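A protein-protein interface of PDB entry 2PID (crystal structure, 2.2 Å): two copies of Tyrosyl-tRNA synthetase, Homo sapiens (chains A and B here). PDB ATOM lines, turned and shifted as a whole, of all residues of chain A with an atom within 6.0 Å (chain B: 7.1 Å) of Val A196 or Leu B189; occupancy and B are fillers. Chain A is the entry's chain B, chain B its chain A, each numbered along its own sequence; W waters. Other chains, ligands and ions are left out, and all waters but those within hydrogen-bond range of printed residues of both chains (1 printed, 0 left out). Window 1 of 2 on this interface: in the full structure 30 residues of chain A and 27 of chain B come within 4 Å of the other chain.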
ATOM      1  N   TYR A 150       8.882 -19.285   1.740  1.00  0.00           N
ATOM      2  CA  TYR A 150       9.887 -18.761   2.668  1.00  0.00           C
ATOM      3  C   TYR A 150      11.000 -17.974   1.989  1.00  0.00           C
ATOM      4  O   TYR A 150      11.568 -17.080   2.599  1.00  0.00           O
ATOM      5  CB  TYR A 150      10.501 -19.870   3.528  1.00  0.00           C
ATOM      6  CG  TYR A 150       9.560 -20.336   4.626  1.00  0.00           C
ATOM      7  CD1 TYR A 150       9.044 -19.412   5.536  1.00  0.00           C
ATOM      8  CD2 TYR A 150       9.134 -21.669   4.742  1.00  0.00           C
ATOM      9  CE1 TYR A 150       8.139 -19.762   6.505  1.00  0.00           C
ATOM     10  CE2 TYR A 150       8.215 -22.027   5.700  1.00  0.00           C
ATOM     11  CZ  TYR A 150       7.716 -21.083   6.576  1.00  0.00           C
ATOM     12  OH  TYR A 150       6.800 -21.470   7.529  1.00  0.00           O
ATOM     13  N   PHE A 158       8.798 -11.071   8.899  1.00  0.00           N
ATOM     14  CA  PHE A 158       8.062 -12.222   9.412  1.00  0.00           C
ATOM     15  C   PHE A 158       7.705 -12.050  10.898  1.00  0.00           C
ATOM     16  O   PHE A 158       6.553 -12.203  11.290  1.00  0.00           O
ATOM     17  CB  PHE A 158       8.879 -13.501   9.225  1.00  0.00           C
ATOM     18  CG  PHE A 158       8.132 -14.751   9.586  1.00  0.00           C
ATOM     19  CD1 PHE A 158       7.206 -15.294   8.710  1.00  0.00           C
ATOM     20  CD2 PHE A 158       8.381 -15.399  10.791  1.00  0.00           C
ATOM     21  CE1 PHE A 158       6.540 -16.476   9.028  1.00  0.00           C
ATOM     22  CE2 PHE A 158       7.726 -16.573  11.121  1.00  0.00           C
ATOM     23  CZ  PHE A 158       6.804 -17.117  10.241  1.00  0.00           C
ATOM     24  N   LEU A 159       8.705 -11.730  11.712  1.00  0.00           N
ATOM     25  CA  LEU A 159       8.492 -11.537  13.146  1.00  0.00           C
ATOM     26  C   LEU A 159       7.479 -10.435  13.415  1.00  0.00           C
ATOM     27  O   LEU A 159       6.644 -10.560  14.302  1.00  0.00           O
ATOM     28  CB  LEU A 159       9.816 -11.206  13.822  1.00  0.00           C
ATOM     29  CG  LEU A 159      10.805 -12.368  13.804  1.00  0.00           C
ATOM     30  CD1 LEU A 159      12.119 -11.917  14.393  1.00  0.00           C
ATOM     31  CD2 LEU A 159      10.229 -13.530  14.601  1.00  0.00           C
ATOM     32  N   VAL A 162       3.729 -11.903  12.132  1.00  0.00           N
ATOM     33  CA  VAL A 162       3.071 -12.952  12.898  1.00  0.00           C
ATOM     34  C   VAL A 162       3.713 -13.203  14.255  1.00  0.00           C
ATOM     35  O   VAL A 162       3.203 -13.981  15.049  1.00  0.00           O
ATOM     36  CB  VAL A 162       3.062 -14.275  12.093  1.00  0.00           C
ATOM     37  CG1 VAL A 162       2.398 -14.055  10.740  1.00  0.00           C
ATOM     38  CG2 VAL A 162       4.461 -14.767  11.886  1.00  0.00           C
ATOM     39  N   GLY A 163       4.824 -12.527  14.523  1.00  0.00           N
ATOM     40  CA  GLY A 163       5.512 -12.711  15.786  1.00  0.00           C
ATOM     41  C   GLY A 163       4.660 -12.425  16.998  1.00  0.00           C
ATOM     42  O   GLY A 163       4.836 -13.053  18.042  1.00  0.00           O
ATOM     43  N   GLY A 164       3.740 -11.473  16.868  1.00  0.00           N
ATOM     44  CA  GLY A 164       2.877 -11.132  17.980  1.00  0.00           C
ATOM     45  C   GLY A 164       1.750 -12.130  18.197  1.00  0.00           C
ATOM     46  O   GLY A 164       1.155 -12.150  19.271  1.00  0.00           O
ATOM     47  N   PHE A 166       2.084 -15.491  17.963  1.00  0.00           N
ATOM     48  CA  PHE A 166       2.591 -16.717  18.540  1.00  0.00           C
ATOM     49  C   PHE A 166       2.917 -16.382  19.982  1.00  0.00           C
ATOM     50  O   PHE A 166       3.632 -15.407  20.262  1.00  0.00           O
ATOM     51  CB  PHE A 166       3.853 -17.185  17.819  1.00  0.00           C
ATOM     52  CG  PHE A 166       3.578 -17.844  16.508  1.00  0.00           C
ATOM     53  CD1 PHE A 166       3.747 -17.149  15.314  1.00  0.00           C
ATOM     54  CD2 PHE A 166       3.134 -19.159  16.471  1.00  0.00           C
ATOM     55  CE1 PHE A 166       3.483 -17.757  14.097  1.00  0.00           C
ATOM     56  CE2 PHE A 166       2.864 -19.780  15.257  1.00  0.00           C
ATOM     57  CZ  PHE A 166       3.041 -19.078  14.065  1.00  0.00           C
ATOM     58  N   ARG A 167       2.368 -17.155  20.908  1.00  0.00           N
ATOM     59  CA  ARG A 167       2.633 -16.915  22.323  1.00  0.00           C
ATOM     60  C   ARG A 167       3.651 -17.932  22.883  1.00  0.00           C
ATOM     61  O   ARG A 167       3.496 -19.148  22.716  1.00  0.00           O
ATOM     62  CB  ARG A 167       1.324 -16.980  23.119  1.00  0.00           C
ATOM     63  CG  ARG A 167       0.195 -16.128  22.524  1.00  0.00           C
ATOM     64  CD  ARG A 167       0.599 -14.662  22.356  1.00  0.00           C
ATOM     65  NE  ARG A 167       0.877 -14.006  23.634  1.00  0.00           N
ATOM     66  CZ  ARG A 167       1.246 -12.728  23.742  1.00  0.00           C
ATOM     67  NH1 ARG A 167       1.376 -11.977  22.652  1.00  0.00           N
ATOM     68  NH2 ARG A 167       1.496 -12.203  24.933  1.00  0.00           N
ATOM     69  N   MET A 168       4.687 -17.417  23.535  1.00  0.00           N
ATOM     70  CA  MET A 168       5.717 -18.256  24.127  1.00  0.00           C
ATOM     71  C   MET A 168       5.115 -19.349  25.010  1.00  0.00           C
ATOM     72  O   MET A 168       5.637 -20.456  25.067  1.00  0.00           O
ATOM     73  CB  MET A 168       6.690 -17.402  24.953  1.00  0.00           C
ATOM     74  CG  MET A 168       7.611 -16.536  24.120  1.00  0.00           C
ATOM     75  SD  MET A 168       8.566 -17.480  22.866  1.00  0.00           S
ATOM     76  CE  MET A 168       9.716 -18.331  23.943  1.00  0.00           C
ATOM     77  N   LEU A 171       3.780 -22.164  22.845  1.00  0.00           N
ATOM     78  CA  LEU A 171       4.950 -22.699  22.142  1.00  0.00           C
ATOM     79  C   LEU A 171       5.851 -23.535  23.061  1.00  0.00           C
ATOM     80  O   LEU A 171       6.385 -24.570  22.650  1.00  0.00           O
ATOM     81  CB  LEU A 171       5.758 -21.539  21.565  1.00  0.00           C
ATOM     82  CG  LEU A 171       5.878 -21.262  20.073  1.00  0.00           C
ATOM     83  CD1 LEU A 171       4.731 -21.827  19.272  1.00  0.00           C
ATOM     84  CD2 LEU A 171       5.998 -19.763  19.919  1.00  0.00           C
ATOM     85  N   PHE A 192      13.645 -24.849  18.291  1.00  0.00           N
ATOM     86  CA  PHE A 192      12.460 -24.266  18.922  1.00  0.00           C
ATOM     87  C   PHE A 192      11.583 -23.584  17.860  1.00  0.00           C
ATOM     88  O   PHE A 192      10.369 -23.698  17.874  1.00  0.00           O
ATOM     89  CB  PHE A 192      12.889 -23.221  19.957  1.00  0.00           C
ATOM     90  CG  PHE A 192      11.750 -22.439  20.537  1.00  0.00           C
ATOM     91  CD1 PHE A 192      10.852 -23.040  21.420  1.00  0.00           C
ATOM     92  CD2 PHE A 192      11.556 -21.102  20.183  1.00  0.00           C
ATOM     93  CE1 PHE A 192       9.766 -22.318  21.948  1.00  0.00           C
ATOM     94  CE2 PHE A 192      10.483 -20.373  20.696  1.00  0.00           C
ATOM     95  CZ  PHE A 192       9.583 -20.978  21.583  1.00  0.00           C
ATOM     96  N   PHE A 193      12.225 -22.863  16.949  1.00  0.00           N
ATOM     97  CA  PHE A 193      11.533 -22.133  15.904  1.00  0.00           C
ATOM     98  C   PHE A 193      10.894 -23.023  14.843  1.00  0.00           C
ATOM     99  O   PHE A 193       9.979 -22.593  14.145  1.00  0.00           O
ATOM    100  CB  PHE A 193      12.491 -21.164  15.208  1.00  0.00           C
ATOM    101  CG  PHE A 193      11.826 -19.883  14.773  1.00  0.00           C
ATOM    102  CD1 PHE A 193      11.756 -18.786  15.644  1.00  0.00           C
ATOM    103  CD2 PHE A 193      11.234 -19.781  13.517  1.00  0.00           C
ATOM    104  CE1 PHE A 193      11.107 -17.605  15.265  1.00  0.00           C
ATOM    105  CE2 PHE A 193      10.578 -18.607  13.125  1.00  0.00           C
ATOM    106  CZ  PHE A 193      10.516 -17.515  14.003  1.00  0.00           C
ATOM    107  N   TYR A 194      11.394 -24.248  14.711  1.00  0.00           N
ATOM    108  CA  TYR A 194      10.878 -25.184  13.720  1.00  0.00           C
ATOM    109  C   TYR A 194       9.340 -25.269  13.715  1.00  0.00           C
ATOM    110  O   TYR A 194       8.707 -25.180  12.651  1.00  0.00           O
ATOM    111  CB  TYR A 194      11.478 -26.574  13.948  1.00  0.00           C
ATOM    112  CG  TYR A 194      11.108 -27.555  12.858  1.00  0.00           C
ATOM    113  CD1 TYR A 194       9.842 -28.138  12.820  1.00  0.00           C
ATOM    114  CD2 TYR A 194      11.996 -27.835  11.822  1.00  0.00           C
ATOM    115  CE1 TYR A 194       9.471 -28.966  11.780  1.00  0.00           C
ATOM    116  CE2 TYR A 194      11.638 -28.663  10.771  1.00  0.00           C
ATOM    117  CZ  TYR A 194      10.383 -29.226  10.753  1.00  0.00           C
ATOM    118  OH  TYR A 194      10.041 -30.061   9.722  1.00  0.00           O
ATOM    119  N   GLN A 195       8.750 -25.423  14.895  1.00  0.00           N
ATOM    120  CA  GLN A 195       7.294 -25.536  15.024  1.00  0.00           C
ATOM    121  C   GLN A 195       6.575 -24.272  14.543  1.00  0.00           C
ATOM    122  O   GLN A 195       5.425 -24.339  14.161  1.00  0.00           O
ATOM    123  CB  GLN A 195       6.896 -25.810  16.480  1.00  0.00           C
ATOM    124  CG  GLN A 195       7.167 -24.661  17.416  1.00  0.00           C
ATOM    125  CD  GLN A 195       6.874 -25.000  18.880  1.00  0.00           C
ATOM    126  OE1 GLN A 195       5.789 -25.483  19.213  1.00  0.00           O
ATOM    127  NE2 GLN A 195       7.843 -24.729  19.760  1.00  0.00           N
ATOM    128  N   VAL A 196       7.241 -23.121  14.598  1.00  0.00           N
ATOM    129  CA  VAL A 196       6.635 -21.879  14.118  1.00  0.00           C
ATOM    130  C   VAL A 196       6.528 -21.952  12.591  1.00  0.00           C
ATOM    131  O   VAL A 196       5.533 -21.500  12.009  1.00  0.00           O
ATOM    132  CB  VAL A 196       7.493 -20.641  14.544  1.00  0.00           C
ATOM    133  CG1 VAL A 196       6.916 -19.324  13.951  1.00  0.00           C
ATOM    134  CG2 VAL A 196       7.505 -20.551  16.067  1.00  0.00           C
ATOM    135  N   LEU A 197       7.546 -22.511  11.933  1.00  0.00           N
ATOM    136  CA  LEU A 197       7.483 -22.636  10.475  1.00  0.00           C
ATOM    137  C   LEU A 197       6.371 -23.601  10.072  1.00  0.00           C
ATOM    138  O   LEU A 197       5.594 -23.299   9.173  1.00  0.00           O
ATOM    139  CB  LEU A 197       8.816 -23.120   9.877  1.00  0.00           C
ATOM    140  CG  LEU A 197      10.041 -22.219  10.103  1.00  0.00           C
ATOM    141  CD1 LEU A 197      11.204 -22.731   9.236  1.00  0.00           C
ATOM    142  CD2 LEU A 197       9.726 -20.756   9.741  1.00  0.00           C
ATOM    143  N   GLN A 198       6.271 -24.750  10.739  1.00  0.00           N
ATOM    144  CA  GLN A 198       5.221 -25.722  10.396  1.00  0.00           C
ATOM    145  C   GLN A 198       3.839 -25.130  10.667  1.00  0.00           C
ATOM    146  O   GLN A 198       2.877 -25.388   9.942  1.00  0.00           O
ATOM    147  CB  GLN A 198       5.388 -27.039  11.184  1.00  0.00           C
ATOM    148  CG  GLN A 198       4.401 -28.154  10.733  1.00  0.00           C
ATOM    149  CD  GLN A 198       4.898 -29.564  11.045  1.00  0.00           C
ATOM    150  OE1 GLN A 198       6.100 -29.808  11.131  1.00  0.00           O
ATOM    151  NE2 GLN A 198       3.968 -30.505  11.184  1.00  0.00           N
ATOM    152  N   ALA A 199       3.746 -24.327  11.720  1.00  0.00           N
ATOM    153  CA  ALA A 199       2.490 -23.706  12.059  1.00  0.00           C
ATOM    154  C   ALA A 199       2.136 -22.688  10.971  1.00  0.00           C
ATOM    155  O   ALA A 199       0.989 -22.600  10.552  1.00  0.00           O
ATOM    156  CB  ALA A 199       2.602 -23.022  13.424  1.00  0.00           C
ATOM    157  N   TYR A 200       3.129 -21.928  10.514  1.00  0.00           N
ATOM    158  CA  TYR A 200       2.905 -20.916   9.485  1.00  0.00           C
ATOM    159  C   TYR A 200       2.515 -21.564   8.162  1.00  0.00           C
ATOM    160  O   TYR A 200       1.657 -21.051   7.427  1.00  0.00           O
ATOM    161  CB  TYR A 200       4.155 -20.037   9.278  1.00  0.00           C
ATOM    162  CG  TYR A 200       3.849 -18.964   8.267  1.00  0.00           C
ATOM    163  CD1 TYR A 200       3.115 -17.811   8.611  1.00  0.00           C
ATOM    164  CD2 TYR A 200       4.253 -19.075   6.940  1.00  0.00           C
ATOM    165  CE1 TYR A 200       2.761 -16.846   7.685  1.00  0.00           C
ATOM    166  CE2 TYR A 200       3.909 -18.132   6.005  1.00  0.00           C
ATOM    167  CZ  TYR A 200       3.153 -17.031   6.366  1.00  0.00           C
ATOM    168  OH  TYR A 200       2.775 -16.114   5.404  1.00  0.00           O
ATOM    169  N   ASP A 201       3.167 -22.679   7.850  1.00  0.00           N
ATOM    170  CA  ASP A 201       2.871 -23.430   6.640  1.00  0.00           C
ATOM    171  C   ASP A 201       1.367 -23.732   6.603  1.00  0.00           C
ATOM    172  O   ASP A 201       0.703 -23.552   5.567  1.00  0.00           O
ATOM    173  CB  ASP A 201       3.618 -24.766   6.643  1.00  0.00           C
ATOM    174  CG  ASP A 201       5.073 -24.652   6.196  1.00  0.00           C
ATOM    175  OD1 ASP A 201       5.534 -23.542   5.844  1.00  0.00           O
ATOM    176  OD2 ASP A 201       5.757 -25.701   6.201  1.00  0.00           O
ATOM    177  N   SER A 226       0.297 -26.516  17.050  1.00  0.00           N
ATOM    178  CA  SER A 226       0.738 -25.122  16.975  1.00  0.00           C
ATOM    179  C   SER A 226       0.059 -24.470  15.783  1.00  0.00           C
ATOM    180  O   SER A 226      -0.329 -23.311  15.852  1.00  0.00           O
ATOM    181  CB  SER A 226       2.259 -25.010  16.842  1.00  0.00           C
ATOM    182  OG  SER A 226       2.901 -25.285  18.074  1.00  0.00           O
ATOM    183  N   LEU B  92       9.762  -4.582  16.414  1.00  0.00           N
ATOM    184  CA  LEU B  92       9.417  -5.687  17.310  1.00  0.00           C
ATOM    185  C   LEU B  92       9.140  -5.183  18.727  1.00  0.00           C
ATOM    186  O   LEU B  92       8.154  -5.568  19.340  1.00  0.00           O
ATOM    187  CB  LEU B  92      10.555  -6.699  17.354  1.00  0.00           C
ATOM    188  CG  LEU B  92      10.480  -7.960  16.498  1.00  0.00           C
ATOM    189  CD1 LEU B  92       9.928  -7.643  15.128  1.00  0.00           C
ATOM    190  CD2 LEU B  92      11.868  -8.580  16.413  1.00  0.00           C
ATOM    191  N   GLU B 101       3.087  -5.550  27.299  1.00  0.00           N
ATOM    192  CA  GLU B 101       3.507  -5.641  25.911  1.00  0.00           C
ATOM    193  C   GLU B 101       3.276  -4.260  25.285  1.00  0.00           C
ATOM    194  O   GLU B 101       2.322  -3.561  25.633  1.00  0.00           O
ATOM    195  CB  GLU B 101       2.672  -6.702  25.186  1.00  0.00           C
ATOM    196  CG  GLU B 101       3.215  -7.142  23.825  1.00  0.00           C
ATOM    197  CD  GLU B 101       2.523  -8.400  23.306  1.00  0.00           C
ATOM    198  OE1 GLU B 101       2.431  -9.392  24.069  1.00  0.00           O
ATOM    199  OE2 GLU B 101       2.079  -8.406  22.137  1.00  0.00           O
ATOM    200  N   LEU B 155      14.274 -15.044   6.475  1.00  0.00           N
ATOM    201  CA  LEU B 155      13.906 -15.826   7.648  1.00  0.00           C
ATOM    202  C   LEU B 155      14.742 -17.074   7.899  1.00  0.00           C
ATOM    203  O   LEU B 155      15.483 -17.163   8.889  1.00  0.00           O
ATOM    204  CB  LEU B 155      12.444 -16.284   7.552  1.00  0.00           C
ATOM    205  CG  LEU B 155      11.576 -16.248   8.813  1.00  0.00           C
ATOM    206  CD1 LEU B 155      10.419 -17.229   8.658  1.00  0.00           C
ATOM    207  CD2 LEU B 155      12.385 -16.562  10.058  1.00  0.00           C
ATOM    208  N   MET B 187       4.562 -13.597  27.035  1.00  0.00           N
ATOM    209  CA  MET B 187       5.187 -12.707  26.074  1.00  0.00           C
ATOM    210  C   MET B 187       5.049 -13.310  24.668  1.00  0.00           C
ATOM    211  O   MET B 187       4.825 -14.525  24.502  1.00  0.00           O
ATOM    212  CB  MET B 187       6.653 -12.478  26.456  1.00  0.00           C
ATOM    213  CG  MET B 187       7.626 -13.402  25.786  1.00  0.00           C
ATOM    214  SD  MET B 187       9.226 -13.474  26.596  1.00  0.00           S
ATOM    215  CE  MET B 187       9.926 -11.848  26.239  1.00  0.00           C
ATOM    216  N   SER B 188       5.159 -12.467  23.654  1.00  0.00           N
ATOM    217  CA  SER B 188       5.030 -12.961  22.292  1.00  0.00           C
ATOM    218  C   SER B 188       6.370 -13.469  21.793  1.00  0.00           C
ATOM    219  O   SER B 188       7.424 -13.179  22.368  1.00  0.00           O
ATOM    220  CB  SER B 188       4.574 -11.850  21.365  1.00  0.00           C
ATOM    221  OG  SER B 188       5.615 -10.905  21.233  1.00  0.00           O
ATOM    222  N   LEU B 189       6.313 -14.224  20.710  1.00  0.00           N
ATOM    223  CA  LEU B 189       7.515 -14.751  20.086  1.00  0.00           C
ATOM    224  C   LEU B 189       8.377 -13.576  19.611  1.00  0.00           C
ATOM    225  O   LEU B 189       9.584 -13.648  19.670  1.00  0.00           O
ATOM    226  CB  LEU B 189       7.137 -15.643  18.901  1.00  0.00           C
ATOM    227  CG  LEU B 189       8.277 -16.114  17.991  1.00  0.00           C
ATOM    228  CD1 LEU B 189       9.234 -16.989  18.794  1.00  0.00           C
ATOM    229  CD2 LEU B 189       7.695 -16.911  16.820  1.00  0.00           C
ATOM    230  N   ALA B 190       7.747 -12.506  19.128  1.00  0.00           N
ATOM    231  CA  ALA B 190       8.487 -11.330  18.681  1.00  0.00           C
ATOM    232  C   ALA B 190       9.285 -10.711  19.837  1.00  0.00           C
ATOM    233  O   ALA B 190      10.461 -10.408  19.684  1.00  0.00           O
ATOM    234  CB  ALA B 190       7.529 -10.291  18.116  1.00  0.00           C
ATOM    235  N   GLU B 191       8.626 -10.496  20.980  1.00  0.00           N
ATOM    236  CA  GLU B 191       9.295  -9.932  22.159  1.00  0.00           C
ATOM    237  C   GLU B 191      10.476 -10.822  22.551  1.00  0.00           C
ATOM    238  O   GLU B 191      11.553 -10.331  22.883  1.00  0.00           O
ATOM    239  CB  GLU B 191       8.345  -9.868  23.357  1.00  0.00           C
ATOM    240  CG  GLU B 191       7.291  -8.765  23.345  1.00  0.00           C
ATOM    241  CD  GLU B 191       6.345  -8.859  24.557  1.00  0.00           C
ATOM    242  OE1 GLU B 191       5.585  -9.848  24.664  1.00  0.00           O
ATOM    243  OE2 GLU B 191       6.365  -7.948  25.405  1.00  0.00           O
ATOM    244  N   PHE B 192      10.254 -12.133  22.512  1.00  0.00           N
ATOM    245  CA  PHE B 192      11.289 -13.091  22.877  1.00  0.00           C
ATOM    246  C   PHE B 192      12.470 -13.052  21.913  1.00  0.00           C
ATOM    247  O   PHE B 192      13.609 -13.167  22.330  1.00  0.00           O
ATOM    248  CB  PHE B 192      10.712 -14.512  22.910  1.00  0.00           C
ATOM    249  CG  PHE B 192      11.746 -15.591  23.204  1.00  0.00           C
ATOM    250  CD1 PHE B 192      12.229 -15.779  24.494  1.00  0.00           C
ATOM    251  CD2 PHE B 192      12.232 -16.410  22.182  1.00  0.00           C
ATOM    252  CE1 PHE B 192      13.172 -16.760  24.771  1.00  0.00           C
ATOM    253  CE2 PHE B 192      13.171 -17.390  22.438  1.00  0.00           C
ATOM    254  CZ  PHE B 192      13.647 -17.569  23.741  1.00  0.00           C
ATOM    255  N   PHE B 193      12.191 -12.871  20.628  1.00  0.00           N
ATOM    256  CA  PHE B 193      13.244 -12.874  19.616  1.00  0.00           C
ATOM    257  C   PHE B 193      14.067 -11.606  19.588  1.00  0.00           C
ATOM    258  O   PHE B 193      15.147 -11.573  19.000  1.00  0.00           O
ATOM    259  CB  PHE B 193      12.636 -13.081  18.232  1.00  0.00           C
ATOM    260  CG  PHE B 193      13.550 -13.796  17.262  1.00  0.00           C
ATOM    261  CD1 PHE B 193      13.554 -15.184  17.187  1.00  0.00           C
ATOM    262  CD2 PHE B 193      14.382 -13.080  16.412  1.00  0.00           C
ATOM    263  CE1 PHE B 193      14.372 -15.852  16.275  1.00  0.00           C
ATOM    264  CE2 PHE B 193      15.206 -13.742  15.497  1.00  0.00           C
ATOM    265  CZ  PHE B 193      15.196 -15.133  15.432  1.00  0.00           C
ATOM    266  N   TYR B 194      13.564 -10.565  20.234  1.00  0.00           N
ATOM    267  CA  TYR B 194      14.249  -9.295  20.239  1.00  0.00           C
ATOM    268  C   TYR B 194      15.712  -9.389  20.623  1.00  0.00           C
ATOM    269  O   TYR B 194      16.582  -8.871  19.906  1.00  0.00           O
ATOM    270  CB  TYR B 194      13.530  -8.314  21.151  1.00  0.00           C
ATOM    271  CG  TYR B 194      14.081  -6.907  21.044  1.00  0.00           C
ATOM    272  CD1 TYR B 194      15.288  -6.561  21.674  1.00  0.00           C
ATOM    273  CD2 TYR B 194      13.422  -5.929  20.280  1.00  0.00           C
ATOM    274  CE1 TYR B 194      15.830  -5.291  21.543  1.00  0.00           C
ATOM    275  CE2 TYR B 194      13.959  -4.639  20.144  1.00  0.00           C
ATOM    276  CZ  TYR B 194      15.163  -4.329  20.775  1.00  0.00           C
ATOM    277  OH  TYR B 194      15.718  -3.073  20.655  1.00  0.00           O
HETATM  278  O   HOH W   1      13.563 -17.458   4.483  1.00  0.00           O
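The side-chain carboxylate (OE1) of Glu B101 lies within salt-bridge range of the guanidinium group (NH2) of Arg A167, 3.1 Å away. O of Met B187 sits at hydrogen-bond distance from N of Met A168, at 3.1 Å. O of Gly A163 lies within hydrogen-bond range of N of Leu B189 (3.3 Å). The backbone NH (N) of Leu B189 lies within hydrogen-bond range of the backbone carbonyl oxygen (O) of Phe A166. The backbone NH of Ala B190 is in hydrogen-bond range of the backbone carbonyl oxygen of Gly A163 (3.2 Å).
OG of Ser B188 sits close to N of Ala B190. The backbone NH (N) of Ser B188 is in hydrogen-bond range of the side-chain carboxylate (OE1) of Glu B191 (2.8 Å). OH of Tyr A150 lies within hydrogen-bond range of O of Leu A197, at 2.7 Å. The backbone carbonyl oxygen of Gly A164 is in hydrogen-bond range of the guanidinium group of Arg A167, at 3.4 Å.
Leu A159 touches Leu B92 (CB to CD1, 3.8 Å). O of Leu A159 touches CB of Ala B190, at 3.9 Å. O of Gly A163 touches CB of Ser B188, at 3.5 Å. CB of Ser B188 touches CA of Gly A164, at 3.9 Å. C of Met B187 touches NH2 of Arg A167, 3.7 Å away. Arg A167 touches Ser B188. Met A168 touches Ser B188. Phe B192 touches Met A168 (CG to CE, 3.5 Å). CG2 of Val A196 touches CD2 of Leu B189, 3.7 Å away. Leu B155 touches Leu A197 (CD1 to CD2, 3.8 Å).
Val A196 touches just one residue of chain B: Leu B189. Leu B189 touches four residues of chain A. Of the printed residues of chain A, Leu B92 touches Leu A159. Of the printed residues of chain A, Glu B101 touches Arg A167. Printed residues of chain A within 4 Å of Phe B193: Leu A159 (3.2 Å) and Phe A193 (3.8 Å). Of the printed residues of chain B, Leu A159 touches Leu B92 (3.8 Å), Ala B190 (3.9 Å) and Phe B193 (3.2 Å). Of the printed residues of chain B, Gly A163 touches Ser B188 (3.5 Å), Leu B189 (3.3 Å) and Ala B190 (3.2 Å). The nearest residue of chain B that does not touch Val A196 is Leu B155 (6.7 Å). The nearest printed residue of chain A that does not touch Ala B190 is Gly A164 (4.2 Å).
Of the 11 printed residues of chain B, 9 touch a printed residue of chain A. Printed residues of chain A that touch a printed residue of chain B: Phe A158, Leu A159, Gly A163, Gly A164, Phe A166, Arg A167, Met A168, Phe A193, Val A196 and Leu A197. Hydrophobic or aromatic side chains of chain A that line the printed part of chain B: Phe A158, Leu A159, Phe A166, Met A168, Phe A193, Val A196 and Leu A197. Among the printed residues, Asp or Glu carboxylates within 4 Å of a Lys or Arg side-chain nitrogen of the other chain: Arg A167 with Glu B101 (3.1 Å).
Phe B193 touches its own counterpart, Phe A193. Of the 20 pairs that touch across the chains among the printed residues, 1 has its exchanged pair printed and touching as well.
Water W1 bridges O of Tyr A150 and N of Leu B155.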
